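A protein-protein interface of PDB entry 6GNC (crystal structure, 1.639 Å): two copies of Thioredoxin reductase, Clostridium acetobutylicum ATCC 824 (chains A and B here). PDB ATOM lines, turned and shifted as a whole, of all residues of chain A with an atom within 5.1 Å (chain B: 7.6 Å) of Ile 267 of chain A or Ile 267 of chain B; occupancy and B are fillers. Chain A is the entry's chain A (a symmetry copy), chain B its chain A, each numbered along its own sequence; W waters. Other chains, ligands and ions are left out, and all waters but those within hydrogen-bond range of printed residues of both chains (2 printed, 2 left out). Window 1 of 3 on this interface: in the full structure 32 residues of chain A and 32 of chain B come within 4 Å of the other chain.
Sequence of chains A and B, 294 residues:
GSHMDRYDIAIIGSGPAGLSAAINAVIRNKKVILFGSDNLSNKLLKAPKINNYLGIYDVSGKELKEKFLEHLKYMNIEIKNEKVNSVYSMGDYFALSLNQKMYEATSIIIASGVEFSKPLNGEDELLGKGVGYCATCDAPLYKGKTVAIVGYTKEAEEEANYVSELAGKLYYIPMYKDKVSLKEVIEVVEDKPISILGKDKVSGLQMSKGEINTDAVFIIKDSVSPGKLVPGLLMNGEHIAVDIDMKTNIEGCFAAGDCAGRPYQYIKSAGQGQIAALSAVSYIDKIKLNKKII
Hydrophobic or aromatic side chains of chain B within 4 Å of the printed part of chain A: Pro 16, Tyr 53, Leu 54, Phe 68, Ile 267, Ala 270 and Ile 275. Along chain B the printed residues that touch a printed residue of chain A span positions 16 to 275. Of the 13 printed residues of chain A, 9 touch a printed residue of chain B. Among the printed residues, 24 pairs touch across the chains. Among the printed residues, no Asp or Glu carboxylate lies within 4 Å of a Lys or Arg side-chain nitrogen of the other chain.
CB of Asn 52 of chain A touches OD1 of Asn 24 of chain B, 3.4 Å away. CG of Leu 54 of chain A touches CD1 of Phe 68 of chain B (3.6 Å). CD1 of Ile 267 of chain A touches OH of Tyr 53 of chain B, 3.3 Å away. Ile 267 of chain B touches Ile 267 of chain A (CG1 to CG1, 3.8 Å). Ile 267 of chain A touches Ala 270 of chain B. Ile 267 of chain A touches Gly 271 of chain B. Ile 267 of chain A touches Gln 274 of chain B (CG2 to OE1, 3.2 Å). Lys 268 of chain A touches Gly 271 of chain B. Ala 270 of chain A touches Ile 267 of chain B. Gly 271 of chain A touches Lys 268 of chain B.
Ser 20 of chain A touches none of the printed residues of chain B. Of the printed residues of chain B, Leu 54 of chain A touches Pro 16 (3.7 Å), Tyr 53 (2.7 Å) and Phe 68 (3.6 Å). Ala 17 of chain B touches none of the printed residues of chain A. Of the printed residues of chain A, Asn 52 of chain B touches Gln 274 (3.5 Å). Printed residues of chain A within 4 Å of Phe 68 of chain B: Leu 54. Ile 267 of chain B touches just these residues of chain A: Tyr 53, Ile 267, Ala 270, Gly 271 and Gln 274. The nearest printed residue of chain B that does not touch Tyr 53 of chain A is Tyr 53 of chain B (4.3 Å).
Tyr 53 of chain A touches Leu 54 of chain B, and with the chains exchanged Leu 54 of chain A touches Tyr 53 of chain B. Ile 267 of chain A touches its own counterpart, Ile 267 of chain B. Ile 267 of chain A touches Gln 274 of chain B, and with the chains exchanged Gln 274 of chain A touches Ile 267 of chain B. 13 positions are printed for both chains. Of the 24 pairs that touch across the chains among the printed residues, 19 have their exchanged pair printed and touching as well.
The side-chain amide oxygen (OD1) of Asn 24 of chain B sits close to the side-chain amide oxygen (OE1) of Gln 265 of chain A, 3.5 Å away. The backbone NH (N) of Lys 268 of chain B lies within hydrogen-bond range of the side-chain amide oxygen (OE1) of Gln 274 of chain A, 2.8 Å away. OE1 of Gln 265 of chain B lies within hydrogen-bond range of NE2 of Gln 274 of chain A (3.4 Å). The side-chain hydroxyl of Tyr 53 of chain B sits at hydrogen-bond distance from the backbone carbonyl oxygen of Leu 54 of chain A, at 2.7 Å. The side-chain amide oxygen of Gln 265 of chain A is in hydrogen-bond range of the side-chain amide nitrogen of Gln 274 of chain B, at 3.4 Å. The backbone carbonyl oxygen (O) of Leu 54 of chain B lies within hydrogen-bond range of the side-chain hydroxyl (OH) of Tyr 53 of chain A (2.7 Å). OE1 of Gln 274 of chain B sits at hydrogen-bond distance from N of Lys 268 of chain A, 2.8 Å away.
OE1 of Gln 265 of chain B is in hydrogen-bond range of ND2 of Asn 52 of chain B (3.0 Å). The side-chain amide nitrogen (ND2) of Asn 52 of chain A lies within hydrogen-bond range of the side-chain amide oxygen (OE1) of Gln 265 of chain A (3.0 Å). The side-chain hydroxyl (OG) of Ser 20 of chain A is in hydrogen-bond range of the backbone carbonyl oxygen (O) of Ala 270 of chain A (2.7 Å). O of Gln 265 of chain B is in hydrogen-bond range of OG of Ser 269 of chain B (2.8 Å).
Water W2 lies within hydrogen-bond range of O of Asn 52 of chain B (2.7 Å), OG of Ser 20 of chain A (2.8 Å) and N of Leu 54 of chain B (2.9 Å). Water W1 lies within hydrogen-bond range of the backbone carbonyl oxygen (O) of Asn 52 of chain A (2.7 Å), the side-chain hydroxyl (OG) of Ser 20 of chain B (2.8 Å) and the backbone NH (N) of Leu 54 of chain A (2.9 Å).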
ATOM      1  N   SER A  20     -24.691  -1.888  -6.959  1.00  0.00           N
ATOM      2  CA  SER A  20     -24.802  -1.285  -5.648  1.00  0.00           C
ATOM      3  C   SER A  20     -24.220   0.126  -5.643  1.00  0.00           C
ATOM      4  O   SER A  20     -24.798   1.043  -5.041  1.00  0.00           O
ATOM      5  CB  SER A  20     -24.111  -2.186  -4.619  1.00  0.00           C
ATOM      6  OG  SER A  20     -24.210  -1.618  -3.344  1.00  0.00           O
ATOM      7  N   ASN A  52     -25.840 -17.519   0.421  1.00  0.00           N
ATOM      8  CA  ASN A  52     -24.987 -16.590   1.160  1.00  0.00           C
ATOM      9  C   ASN A  52     -25.206 -15.069   0.931  1.00  0.00           C
ATOM     10  O   ASN A  52     -24.329 -14.290   1.284  1.00  0.00           O
ATOM     11  CB  ASN A  52     -23.512 -16.945   0.968  1.00  0.00           C
ATOM     12  CG  ASN A  52     -23.030 -16.690  -0.437  1.00  0.00           C
ATOM     13  OD1 ASN A  52     -23.821 -16.479  -1.345  1.00  0.00           O
ATOM     14  ND2 ASN A  52     -21.720 -16.705  -0.619  1.00  0.00           N
ATOM     15  N   TYR A  53     -26.314 -14.635   0.321  1.00  0.00           N
ATOM     16  CA  TYR A  53     -26.564 -13.221   0.139  1.00  0.00           C
ATOM     17  C   TYR A  53     -27.616 -12.931   1.201  1.00  0.00           C
ATOM     18  O   TYR A  53     -28.749 -13.354   1.054  1.00  0.00           O
ATOM     19  CB  TYR A  53     -27.124 -12.984  -1.260  1.00  0.00           C
ATOM     20  CG  TYR A  53     -27.159 -11.543  -1.689  1.00  0.00           C
ATOM     21  CD1 TYR A  53     -28.234 -10.735  -1.374  1.00  0.00           C
ATOM     22  CD2 TYR A  53     -26.119 -10.995  -2.419  1.00  0.00           C
ATOM     23  CE1 TYR A  53     -28.271  -9.416  -1.767  1.00  0.00           C
ATOM     24  CE2 TYR A  53     -26.146  -9.677  -2.817  1.00  0.00           C
ATOM     25  CZ  TYR A  53     -27.224  -8.893  -2.489  1.00  0.00           C
ATOM     26  OH  TYR A  53     -27.257  -7.582  -2.881  1.00  0.00           O
ATOM     27  N   LEU A  54     -27.284 -12.148   2.221  1.00  0.00           N
ATOM     28  CA  LEU A  54     -28.218 -11.936   3.316  1.00  0.00           C
ATOM     29  C   LEU A  54     -29.547 -11.316   2.861  1.00  0.00           C
ATOM     30  O   LEU A  54     -29.553 -10.305   2.176  1.00  0.00           O
ATOM     31  CB  LEU A  54     -27.575 -11.038   4.368  1.00  0.00           C
ATOM     32  CG  LEU A  54     -28.439 -10.676   5.572  1.00  0.00           C
ATOM     33  CD1 LEU A  54     -28.781 -11.917   6.383  1.00  0.00           C
ATOM     34  CD2 LEU A  54     -27.729  -9.650   6.435  1.00  0.00           C
ATOM     35  N   GLN A 265     -17.230 -12.889  -3.828  1.00  0.00           N
ATOM     36  CA  GLN A 265     -18.602 -13.119  -3.400  1.00  0.00           C
ATOM     37  C   GLN A 265     -19.514 -11.944  -3.728  1.00  0.00           C
ATOM     38  O   GLN A 265     -19.064 -10.787  -3.806  1.00  0.00           O
ATOM     39  CB  GLN A 265     -18.675 -13.355  -1.882  1.00  0.00           C
ATOM     40  CG  GLN A 265     -17.729 -14.392  -1.316  1.00  0.00           C
ATOM     41  CD  GLN A 265     -18.350 -15.760  -1.275  1.00  0.00           C
ATOM     42  OE1 GLN A 265     -18.820 -16.243  -0.218  1.00  0.00           O
ATOM     43  NE2 GLN A 265     -18.371 -16.419  -2.419  1.00  0.00           N
ATOM     44  N   TYR A 266     -20.816 -12.240  -3.862  1.00  0.00           N
ATOM     45  CA  TYR A 266     -21.773 -11.224  -4.309  1.00  0.00           C
ATOM     46  C   TYR A 266     -21.931 -10.104  -3.284  1.00  0.00           C
ATOM     47  O   TYR A 266     -21.915  -8.917  -3.634  1.00  0.00           O
ATOM     48  CB  TYR A 266     -23.163 -11.828  -4.577  1.00  0.00           C
ATOM     49  CG  TYR A 266     -23.267 -12.917  -5.616  1.00  0.00           C
ATOM     50  CD1 TYR A 266     -22.922 -12.690  -6.953  1.00  0.00           C
ATOM     51  CD2 TYR A 266     -23.748 -14.160  -5.273  1.00  0.00           C
ATOM     52  CE1 TYR A 266     -23.027 -13.715  -7.900  1.00  0.00           C
ATOM     53  CE2 TYR A 266     -23.844 -15.180  -6.194  1.00  0.00           C
ATOM     54  CZ  TYR A 266     -23.496 -14.955  -7.512  1.00  0.00           C
ATOM     55  OH  TYR A 266     -23.613 -15.992  -8.415  1.00  0.00           O
ATOM     56  N   ILE A 267     -22.146 -10.444  -2.000  1.00  0.00           N
ATOM     57  CA  ILE A 267     -22.549  -9.363  -1.100  1.00  0.00           C
ATOM     58  C   ILE A 267     -21.325  -8.549  -0.666  1.00  0.00           C
ATOM     59  O   ILE A 267     -21.428  -7.335  -0.460  1.00  0.00           O
ATOM     60  CB  ILE A 267     -23.408  -9.902   0.072  1.00  0.00           C
ATOM     61  CG1 ILE A 267     -24.283  -8.754   0.614  1.00  0.00           C
ATOM     62  CG2 ILE A 267     -22.605 -10.537   1.138  1.00  0.00           C
ATOM     63  CD1 ILE A 267     -25.568  -9.160   1.359  1.00  0.00           C
ATOM     64  N   LYS A 268     -20.147  -9.187  -0.553  1.00  0.00           N
ATOM     65  CA  LYS A 268     -18.895  -8.443  -0.440  1.00  0.00           C
ATOM     66  C   LYS A 268     -18.784  -7.431  -1.574  1.00  0.00           C
ATOM     67  O   LYS A 268     -18.424  -6.277  -1.338  1.00  0.00           O
ATOM     68  CB  LYS A 268     -17.710  -9.417  -0.472  1.00  0.00           C
ATOM     69  CG  LYS A 268     -16.310  -8.822  -0.395  1.00  0.00           C
ATOM     70  CD  LYS A 268     -15.768  -8.329  -1.675  1.00  0.00           C
ATOM     71  CE  LYS A 268     -14.255  -8.527  -1.697  1.00  0.00           C
ATOM     72  NZ  LYS A 268     -13.833  -8.137  -3.050  1.00  0.00           N
ATOM     73  N   SER A 269     -19.112  -7.851  -2.793  1.00  0.00           N
ATOM     74  CA  SER A 269     -18.997  -6.941  -3.936  1.00  0.00           C
ATOM     75  C   SER A 269     -19.975  -5.788  -3.810  1.00  0.00           C
ATOM     76  O   SER A 269     -19.622  -4.627  -4.074  1.00  0.00           O
ATOM     77  CB  SER A 269     -19.219  -7.687  -5.258  1.00  0.00           C
ATOM     78  OG  SER A 269     -18.212  -8.657  -5.452  1.00  0.00           O
ATOM     79  N   ALA A 270     -21.221  -6.078  -3.456  1.00  0.00           N
ATOM     80  CA  ALA A 270     -22.216  -5.024  -3.262  1.00  0.00           C
ATOM     81  C   ALA A 270     -21.804  -4.064  -2.162  1.00  0.00           C
ATOM     82  O   ALA A 270     -22.004  -2.852  -2.281  1.00  0.00           O
ATOM     83  CB  ALA A 270     -23.577  -5.656  -2.950  1.00  0.00           C
ATOM     84  N   GLY A 271     -21.263  -4.578  -1.050  1.00  0.00           N
ATOM     85  CA  GLY A 271     -20.817  -3.690   0.005  1.00  0.00           C
ATOM     86  C   GLY A 271     -19.697  -2.764  -0.445  1.00  0.00           C
ATOM     87  O   GLY A 271     -19.700  -1.574  -0.128  1.00  0.00           O
ATOM     88  N   GLN A 272     -18.729  -3.304  -1.189  1.00  0.00           N
ATOM     89  CA  GLN A 272     -17.628  -2.472  -1.668  1.00  0.00           C
ATOM     90  C   GLN A 272     -18.130  -1.457  -2.672  1.00  0.00           C
ATOM     91  O   GLN A 272     -17.622  -0.319  -2.724  1.00  0.00           O
ATOM     92  CB  GLN A 272     -16.535  -3.338  -2.286  1.00  0.00           C
ATOM     93  CG  GLN A 272     -15.726  -4.084  -1.216  1.00  0.00           C
ATOM     94  CD  GLN A 272     -14.578  -4.889  -1.760  1.00  0.00           C
ATOM     95  OE1 GLN A 272     -14.576  -5.307  -2.908  1.00  0.00           O
ATOM     96  NE2 GLN A 272     -13.600  -5.170  -0.891  1.00  0.00           N
ATOM     97  N   GLN A 274     -20.976   0.021  -2.611  1.00  0.00           N
ATOM     98  CA  GLN A 274     -21.555   1.090  -1.819  1.00  0.00           C
ATOM     99  C   GLN A 274     -20.475   1.968  -1.207  1.00  0.00           C
ATOM    100  O   GLN A 274     -20.588   3.201  -1.235  1.00  0.00           O
ATOM    101  CB  GLN A 274     -22.479   0.448  -0.770  1.00  0.00           C
ATOM    102  CG  GLN A 274     -23.037   1.414   0.218  1.00  0.00           C
ATOM    103  CD  GLN A 274     -23.960   0.731   1.152  1.00  0.00           C
ATOM    104  OE1 GLN A 274     -23.518  -0.090   1.961  1.00  0.00           O
ATOM    105  NE2 GLN A 274     -25.253   1.014   1.040  1.00  0.00           N
ATOM    106  N   PRO B  16     -26.692  -6.704  10.385  1.00  0.00           N
ATOM    107  CA  PRO B  16     -26.338  -7.354   9.113  1.00  0.00           C
ATOM    108  C   PRO B  16     -24.912  -7.869   9.039  1.00  0.00           C
ATOM    109  O   PRO B  16     -24.682  -8.892   8.376  1.00  0.00           O
ATOM    110  CB  PRO B  16     -26.587  -6.243   8.073  1.00  0.00           C
ATOM    111  CG  PRO B  16     -26.551  -4.959   8.858  1.00  0.00           C
ATOM    112  CD  PRO B  16     -27.198  -5.333  10.189  1.00  0.00           C
ATOM    113  N   ALA B  17     -23.939  -7.205   9.673  1.00  0.00           N
ATOM    114  CA  ALA B  17     -22.578  -7.727   9.661  1.00  0.00           C
ATOM    115  C   ALA B  17     -22.516  -9.103  10.339  1.00  0.00           C
ATOM    116  O   ALA B  17     -22.005 -10.060   9.755  1.00  0.00           O
ATOM    117  CB  ALA B  17     -21.612  -6.757  10.340  1.00  0.00           C
ATOM    118  N   SER B  20     -24.574 -11.834   8.299  1.00  0.00           N
ATOM    119  CA  SER B  20     -23.888 -12.261   7.099  1.00  0.00           C
ATOM    120  C   SER B  20     -22.675 -13.123   7.437  1.00  0.00           C
ATOM    121  O   SER B  20     -22.419 -14.138   6.774  1.00  0.00           O
ATOM    122  CB  SER B  20     -23.495 -11.029   6.278  1.00  0.00           C
ATOM    123  OG  SER B  20     -22.831 -11.424   5.110  1.00  0.00           O
ATOM    124  N   ASN B  24     -22.313 -17.178   6.322  1.00  0.00           N
ATOM    125  CA  ASN B  24     -21.196 -17.603   5.496  1.00  0.00           C
ATOM    126  C   ASN B  24     -20.325 -18.625   6.222  1.00  0.00           C
ATOM    127  O   ASN B  24     -19.823 -19.565   5.599  1.00  0.00           O
ATOM    128  CB  ASN B  24     -20.387 -16.391   5.071  1.00  0.00           C
ATOM    129  CG  ASN B  24     -20.971 -15.737   3.831  1.00  0.00           C
ATOM    130  OD1 ASN B  24     -20.671 -16.162   2.734  1.00  0.00           O
ATOM    131  ND2 ASN B  24     -21.868 -14.765   4.017  1.00  0.00           N
ATOM    132  N   ASN B  52     -31.416   1.352  -0.613  1.00  0.00           N
ATOM    133  CA  ASN B  52     -30.006   1.115  -0.919  1.00  0.00           C
ATOM    134  C   ASN B  52     -29.429  -0.296  -0.621  1.00  0.00           C
ATOM    135  O   ASN B  52     -28.213  -0.434  -0.572  1.00  0.00           O
ATOM    136  CB  ASN B  52     -29.129   2.190  -0.275  1.00  0.00           C
ATOM    137  CG  ASN B  52     -29.097   2.092   1.229  1.00  0.00           C
ATOM    138  OD1 ASN B  52     -29.899   1.394   1.830  1.00  0.00           O
ATOM    139  ND2 ASN B  52     -28.159   2.795   1.841  1.00  0.00           N
ATOM    140  N   TYR B  53     -30.253  -1.321  -0.382  1.00  0.00           N
ATOM    141  CA  TYR B  53     -29.742  -2.656  -0.150  1.00  0.00           C
ATOM    142  C   TYR B  53     -30.033  -3.356  -1.469  1.00  0.00           C
ATOM    143  O   TYR B  53     -31.184  -3.632  -1.760  1.00  0.00           O
ATOM    144  CB  TYR B  53     -30.519  -3.301   0.994  1.00  0.00           C
ATOM    145  CG  TYR B  53     -29.911  -4.567   1.532  1.00  0.00           C
ATOM    146  CD1 TYR B  53     -30.194  -5.791   0.957  1.00  0.00           C
ATOM    147  CD2 TYR B  53     -29.062  -4.538   2.625  1.00  0.00           C
ATOM    148  CE1 TYR B  53     -29.642  -6.952   1.449  1.00  0.00           C
ATOM    149  CE2 TYR B  53     -28.505  -5.693   3.124  1.00  0.00           C
ATOM    150  CZ  TYR B  53     -28.798  -6.897   2.533  1.00  0.00           C
ATOM    151  OH  TYR B  53     -28.246  -8.049   3.025  1.00  0.00           O
ATOM    152  N   LEU B  54     -29.008  -3.725  -2.229  1.00  0.00           N
ATOM    153  CA  LEU B  54     -29.241  -4.293  -3.548  1.00  0.00           C
ATOM    154  C   LEU B  54     -30.081  -5.578  -3.509  1.00  0.00           C
ATOM    155  O   LEU B  54     -29.771  -6.495  -2.765  1.00  0.00           O
ATOM    156  CB  LEU B  54     -27.903  -4.585  -4.220  1.00  0.00           C
ATOM    157  CG  LEU B  54     -27.963  -5.230  -5.601  1.00  0.00           C
ATOM    158  CD1 LEU B  54     -28.622  -4.296  -6.603  1.00  0.00           C
ATOM    159  CD2 LEU B  54     -26.568  -5.612  -6.061  1.00  0.00           C
ATOM    160  N   GLY B  55     -31.115  -5.651  -4.349  1.00  0.00           N
ATOM    161  CA  GLY B  55     -32.002  -6.800  -4.409  1.00  0.00           C
ATOM    162  C   GLY B  55     -33.272  -6.789  -3.554  1.00  0.00           C
ATOM    163  O   GLY B  55     -34.190  -7.541  -3.860  1.00  0.00           O
ATOM    164  N   ILE B  56     -33.362  -5.966  -2.507  1.00  0.00           N
ATOM    165  CA  ILE B  56     -34.575  -5.875  -1.715  1.00  0.00           C
ATOM    166  C   ILE B  56     -34.863  -4.384  -1.670  1.00  0.00           C
ATOM    167  O   ILE B  56     -34.128  -3.648  -1.031  1.00  0.00           O
ATOM    168  CB  ILE B  56     -34.355  -6.408  -0.291  1.00  0.00           C
ATOM    169  CG1 ILE B  56     -33.722  -7.796  -0.339  1.00  0.00           C
ATOM    170  CG2 ILE B  56     -35.665  -6.452   0.475  1.00  0.00           C
ATOM    171  CD1 ILE B  56     -33.397  -8.364   1.022  1.00  0.00           C
ATOM    172  N   LEU B  64     -37.314  -5.459   6.302  1.00  0.00           N
ATOM    173  CA  LEU B  64     -35.963  -5.949   6.050  1.00  0.00           C
ATOM    174  C   LEU B  64     -35.498  -6.902   7.170  1.00  0.00           C
ATOM    175  O   LEU B  64     -34.903  -7.932   6.882  1.00  0.00           O
ATOM    176  CB  LEU B  64     -34.978  -4.792   5.910  1.00  0.00           C
ATOM    177  CG  LEU B  64     -33.579  -5.206   5.453  1.00  0.00           C
ATOM    178  CD1 LEU B  64     -33.641  -5.983   4.150  1.00  0.00           C
ATOM    179  CD2 LEU B  64     -32.679  -3.993   5.312  1.00  0.00           C
ATOM    180  N   PHE B  68     -34.313 -10.911   6.915  1.00  0.00           N
ATOM    181  CA  PHE B  68     -33.090 -11.420   7.520  1.00  0.00           C
ATOM    182  C   PHE B  68     -33.410 -12.601   8.432  1.00  0.00           C
ATOM    183  O   PHE B  68     -32.726 -13.627   8.391  1.00  0.00           O
ATOM    184  CB  PHE B  68     -32.414 -10.303   8.308  1.00  0.00           C
ATOM    185  CG  PHE B  68     -31.776  -9.217   7.477  1.00  0.00           C
ATOM    186  CD1 PHE B  68     -31.675  -9.280   6.077  1.00  0.00           C
ATOM    187  CD2 PHE B  68     -31.242  -8.129   8.123  1.00  0.00           C
ATOM    188  CE1 PHE B  68     -31.044  -8.250   5.358  1.00  0.00           C
ATOM    189  CE2 PHE B  68     -30.631  -7.109   7.409  1.00  0.00           C
ATOM    190  CZ  PHE B  68     -30.531  -7.168   6.033  1.00  0.00           C
ATOM    191  N   TYR B 264     -21.760   4.150   7.467  1.00  0.00           N
ATOM    192  CA  TYR B 264     -22.615   3.265   8.227  1.00  0.00           C
ATOM    193  C   TYR B 264     -23.792   2.900   7.335  1.00  0.00           C
ATOM    194  O   TYR B 264     -24.731   3.671   7.180  1.00  0.00           O
ATOM    195  CB  TYR B 264     -23.113   3.952   9.498  1.00  0.00           C
ATOM    196  CG  TYR B 264     -22.026   4.395  10.454  1.00  0.00           C
ATOM    197  CD1 TYR B 264     -20.886   3.631  10.648  1.00  0.00           C
ATOM    198  CD2 TYR B 264     -22.159   5.562  11.186  1.00  0.00           C
ATOM    199  CE1 TYR B 264     -19.901   4.031  11.529  1.00  0.00           C
ATOM    200  CE2 TYR B 264     -21.181   5.967  12.071  1.00  0.00           C
ATOM    201  CZ  TYR B 264     -20.054   5.198  12.239  1.00  0.00           C
ATOM    202  OH  TYR B 264     -19.083   5.602  13.119  1.00  0.00           O
ATOM    203  N   GLN B 265     -23.728   1.709   6.761  1.00  0.00           N
ATOM    204  CA  GLN B 265     -24.763   1.203   5.872  1.00  0.00           C
ATOM    205  C   GLN B 265     -24.939  -0.306   5.990  1.00  0.00           C
ATOM    206  O   GLN B 265     -23.993  -1.035   6.336  1.00  0.00           O
ATOM    207  CB  GLN B 265     -24.431   1.518   4.403  1.00  0.00           C
ATOM    208  CG  GLN B 265     -24.073   2.953   4.087  1.00  0.00           C
ATOM    209  CD  GLN B 265     -25.278   3.763   3.696  1.00  0.00           C
ATOM    210  OE1 GLN B 265     -25.542   4.021   2.499  1.00  0.00           O
ATOM    211  NE2 GLN B 265     -26.039   4.183   4.690  1.00  0.00           N
ATOM    212  N   TYR B 266     -26.147  -0.777   5.644  1.00  0.00           N
ATOM    213  CA  TYR B 266     -26.484  -2.189   5.842  1.00  0.00           C
ATOM    214  C   TYR B 266     -25.652  -3.103   4.946  1.00  0.00           C
ATOM    215  O   TYR B 266     -25.116  -4.121   5.403  1.00  0.00           O
ATOM    216  CB  TYR B 266     -27.972  -2.467   5.558  1.00  0.00           C
ATOM    217  CG  TYR B 266     -28.993  -1.722   6.382  1.00  0.00           C
ATOM    218  CD1 TYR B 266     -29.059  -1.863   7.772  1.00  0.00           C
ATOM    219  CD2 TYR B 266     -29.920  -0.910   5.768  1.00  0.00           C
ATOM    220  CE1 TYR B 266     -30.016  -1.163   8.515  1.00  0.00           C
ATOM    221  CE2 TYR B 266     -30.859  -0.207   6.491  1.00  0.00           C
ATOM    222  CZ  TYR B 266     -30.916  -0.342   7.865  1.00  0.00           C
ATOM    223  OH  TYR B 266     -31.875   0.365   8.562  1.00  0.00           O
ATOM    224  N   ILE B 267     -25.565  -2.803   3.638  1.00  0.00           N
ATOM    225  CA  ILE B 267     -24.985  -3.829   2.771  1.00  0.00           C
ATOM    226  C   ILE B 267     -23.455  -3.801   2.866  1.00  0.00           C
ATOM    227  O   ILE B 267     -22.807  -4.848   2.765  1.00  0.00           O
ATOM    228  CB  ILE B 267     -25.540  -3.723   1.329  1.00  0.00           C
ATOM    229  CG1 ILE B 267     -25.407  -5.099   0.644  1.00  0.00           C
ATOM    230  CG2 ILE B 267     -24.905  -2.648   0.538  1.00  0.00           C
ATOM    231  CD1 ILE B 267     -26.363  -5.378  -0.531  1.00  0.00           C
ATOM    232  N   LYS B 268     -22.856  -2.619   3.094  1.00  0.00           N
ATOM    233  CA  LYS B 268     -21.452  -2.550   3.490  1.00  0.00           C
ATOM    234  C   LYS B 268     -21.204  -3.452   4.693  1.00  0.00           C
ATOM    235  O   LYS B 268     -20.222  -4.196   4.715  1.00  0.00           O
ATOM    236  CB  LYS B 268     -21.079  -1.099   3.822  1.00  0.00           C
ATOM    237  CG  LYS B 268     -19.654  -0.830   4.286  1.00  0.00           C
ATOM    238  CD  LYS B 268     -19.404  -1.081   5.717  1.00  0.00           C
ATOM    239  CE  LYS B 268     -18.355  -0.099   6.231  1.00  0.00           C
ATOM    240  NZ  LYS B 268     -18.278  -0.336   7.680  1.00  0.00           N
ATOM    241  N   SER B 269     -22.097  -3.405   5.678  1.00  0.00           N
ATOM    242  CA  SER B 269     -21.903  -4.221   6.880  1.00  0.00           C
ATOM    243  C   SER B 269     -21.989  -5.700   6.550  1.00  0.00           C
ATOM    244  O   SER B 269     -21.178  -6.504   7.037  1.00  0.00           O
ATOM    245  CB  SER B 269     -22.927  -3.856   7.963  1.00  0.00           C
ATOM    246  OG  SER B 269     -22.744  -2.522   8.386  1.00  0.00           O
ATOM    247  N   ALA B 270     -22.984  -6.096   5.767  1.00  0.00           N
ATOM    248  CA  ALA B 270     -23.114  -7.493   5.357  1.00  0.00           C
ATOM    249  C   ALA B 270     -21.903  -7.957   4.568  1.00  0.00           C
ATOM    250  O   ALA B 270     -21.441  -9.089   4.737  1.00  0.00           O
ATOM    251  CB  ALA B 270     -24.396  -7.671   4.538  1.00  0.00           C
ATOM    252  N   GLY B 271     -21.388  -7.120   3.658  1.00  0.00           N
ATOM    253  CA  GLY B 271     -20.207  -7.510   2.915  1.00  0.00           C
ATOM    254  C   GLY B 271     -18.996  -7.723   3.813  1.00  0.00           C
ATOM    255  O   GLY B 271     -18.246  -8.685   3.638  1.00  0.00           O
ATOM    256  N   GLN B 272     -18.796  -6.825   4.781  1.00  0.00           N
ATOM    257  CA  GLN B 272     -17.661  -6.973   5.688  1.00  0.00           C
ATOM    258  C   GLN B 272     -17.838  -8.196   6.562  1.00  0.00           C
ATOM    259  O   GLN B 272     -16.850  -8.876   6.901  1.00  0.00           O
ATOM    260  CB  GLN B 272     -17.499  -5.723   6.547  1.00  0.00           C
ATOM    261  CG  GLN B 272     -16.918  -4.552   5.744  1.00  0.00           C
ATOM    262  CD  GLN B 272     -16.655  -3.315   6.558  1.00  0.00           C
ATOM    263  OE1 GLN B 272     -17.270  -3.085   7.589  1.00  0.00           O
ATOM    264  NE2 GLN B 272     -15.760  -2.461   6.048  1.00  0.00           N
ATOM    265  N   GLY B 273     -19.072  -8.502   6.939  1.00  0.00           N
ATOM    266  CA  GLY B 273     -19.296  -9.690   7.750  1.00  0.00           C
ATOM    267  C   GLY B 273     -18.907 -10.937   6.992  1.00  0.00           C
ATOM    268  O   GLY B 273     -18.320 -11.869   7.550  1.00  0.00           O
ATOM    269  N   GLN B 274     -19.207 -10.964   5.693  1.00  0.00           N
ATOM    270  CA  GLN B 274     -18.805 -12.087   4.867  1.00  0.00           C
ATOM    271  C   GLN B 274     -17.291 -12.171   4.752  1.00  0.00           C
ATOM    272  O   GLN B 274     -16.721 -13.264   4.868  1.00  0.00           O
ATOM    273  CB  GLN B 274     -19.508 -11.943   3.506  1.00  0.00           C
ATOM    274  CG  GLN B 274     -19.078 -12.948   2.493  1.00  0.00           C
ATOM    275  CD  GLN B 274     -19.842 -12.781   1.236  1.00  0.00           C
ATOM    276  OE1 GLN B 274     -19.671 -11.772   0.545  1.00  0.00           O
ATOM    277  NE2 GLN B 274     -20.721 -13.728   0.932  1.00  0.00           N
ATOM    278  N   ILE B 275     -16.609 -11.042   4.552  1.00  0.00           N
ATOM    279  CA  ILE B 275     -15.152 -11.053   4.494  1.00  0.00           C
ATOM    280  C   ILE B 275     -14.590 -11.598   5.803  1.00  0.00           C
ATOM    281  O   ILE B 275     -13.685 -12.436   5.807  1.00  0.00           O
ATOM    282  CB  ILE B 275     -14.598  -9.650   4.233  1.00  0.00           C
ATOM    283  CG1 ILE B 275     -15.047  -9.128   2.855  1.00  0.00           C
ATOM    284  CG2 ILE B 275     -13.061  -9.639   4.353  1.00  0.00           C
ATOM    285  CD1 ILE B 275     -14.661  -7.657   2.689  1.00  0.00           C
HETATM  286  O   HOH W   1     -24.629 -12.654   3.391  1.00  0.00           O
HETATM  287  O   HOH W   2     -26.843  -1.743  -2.475  1.00  0.00           O
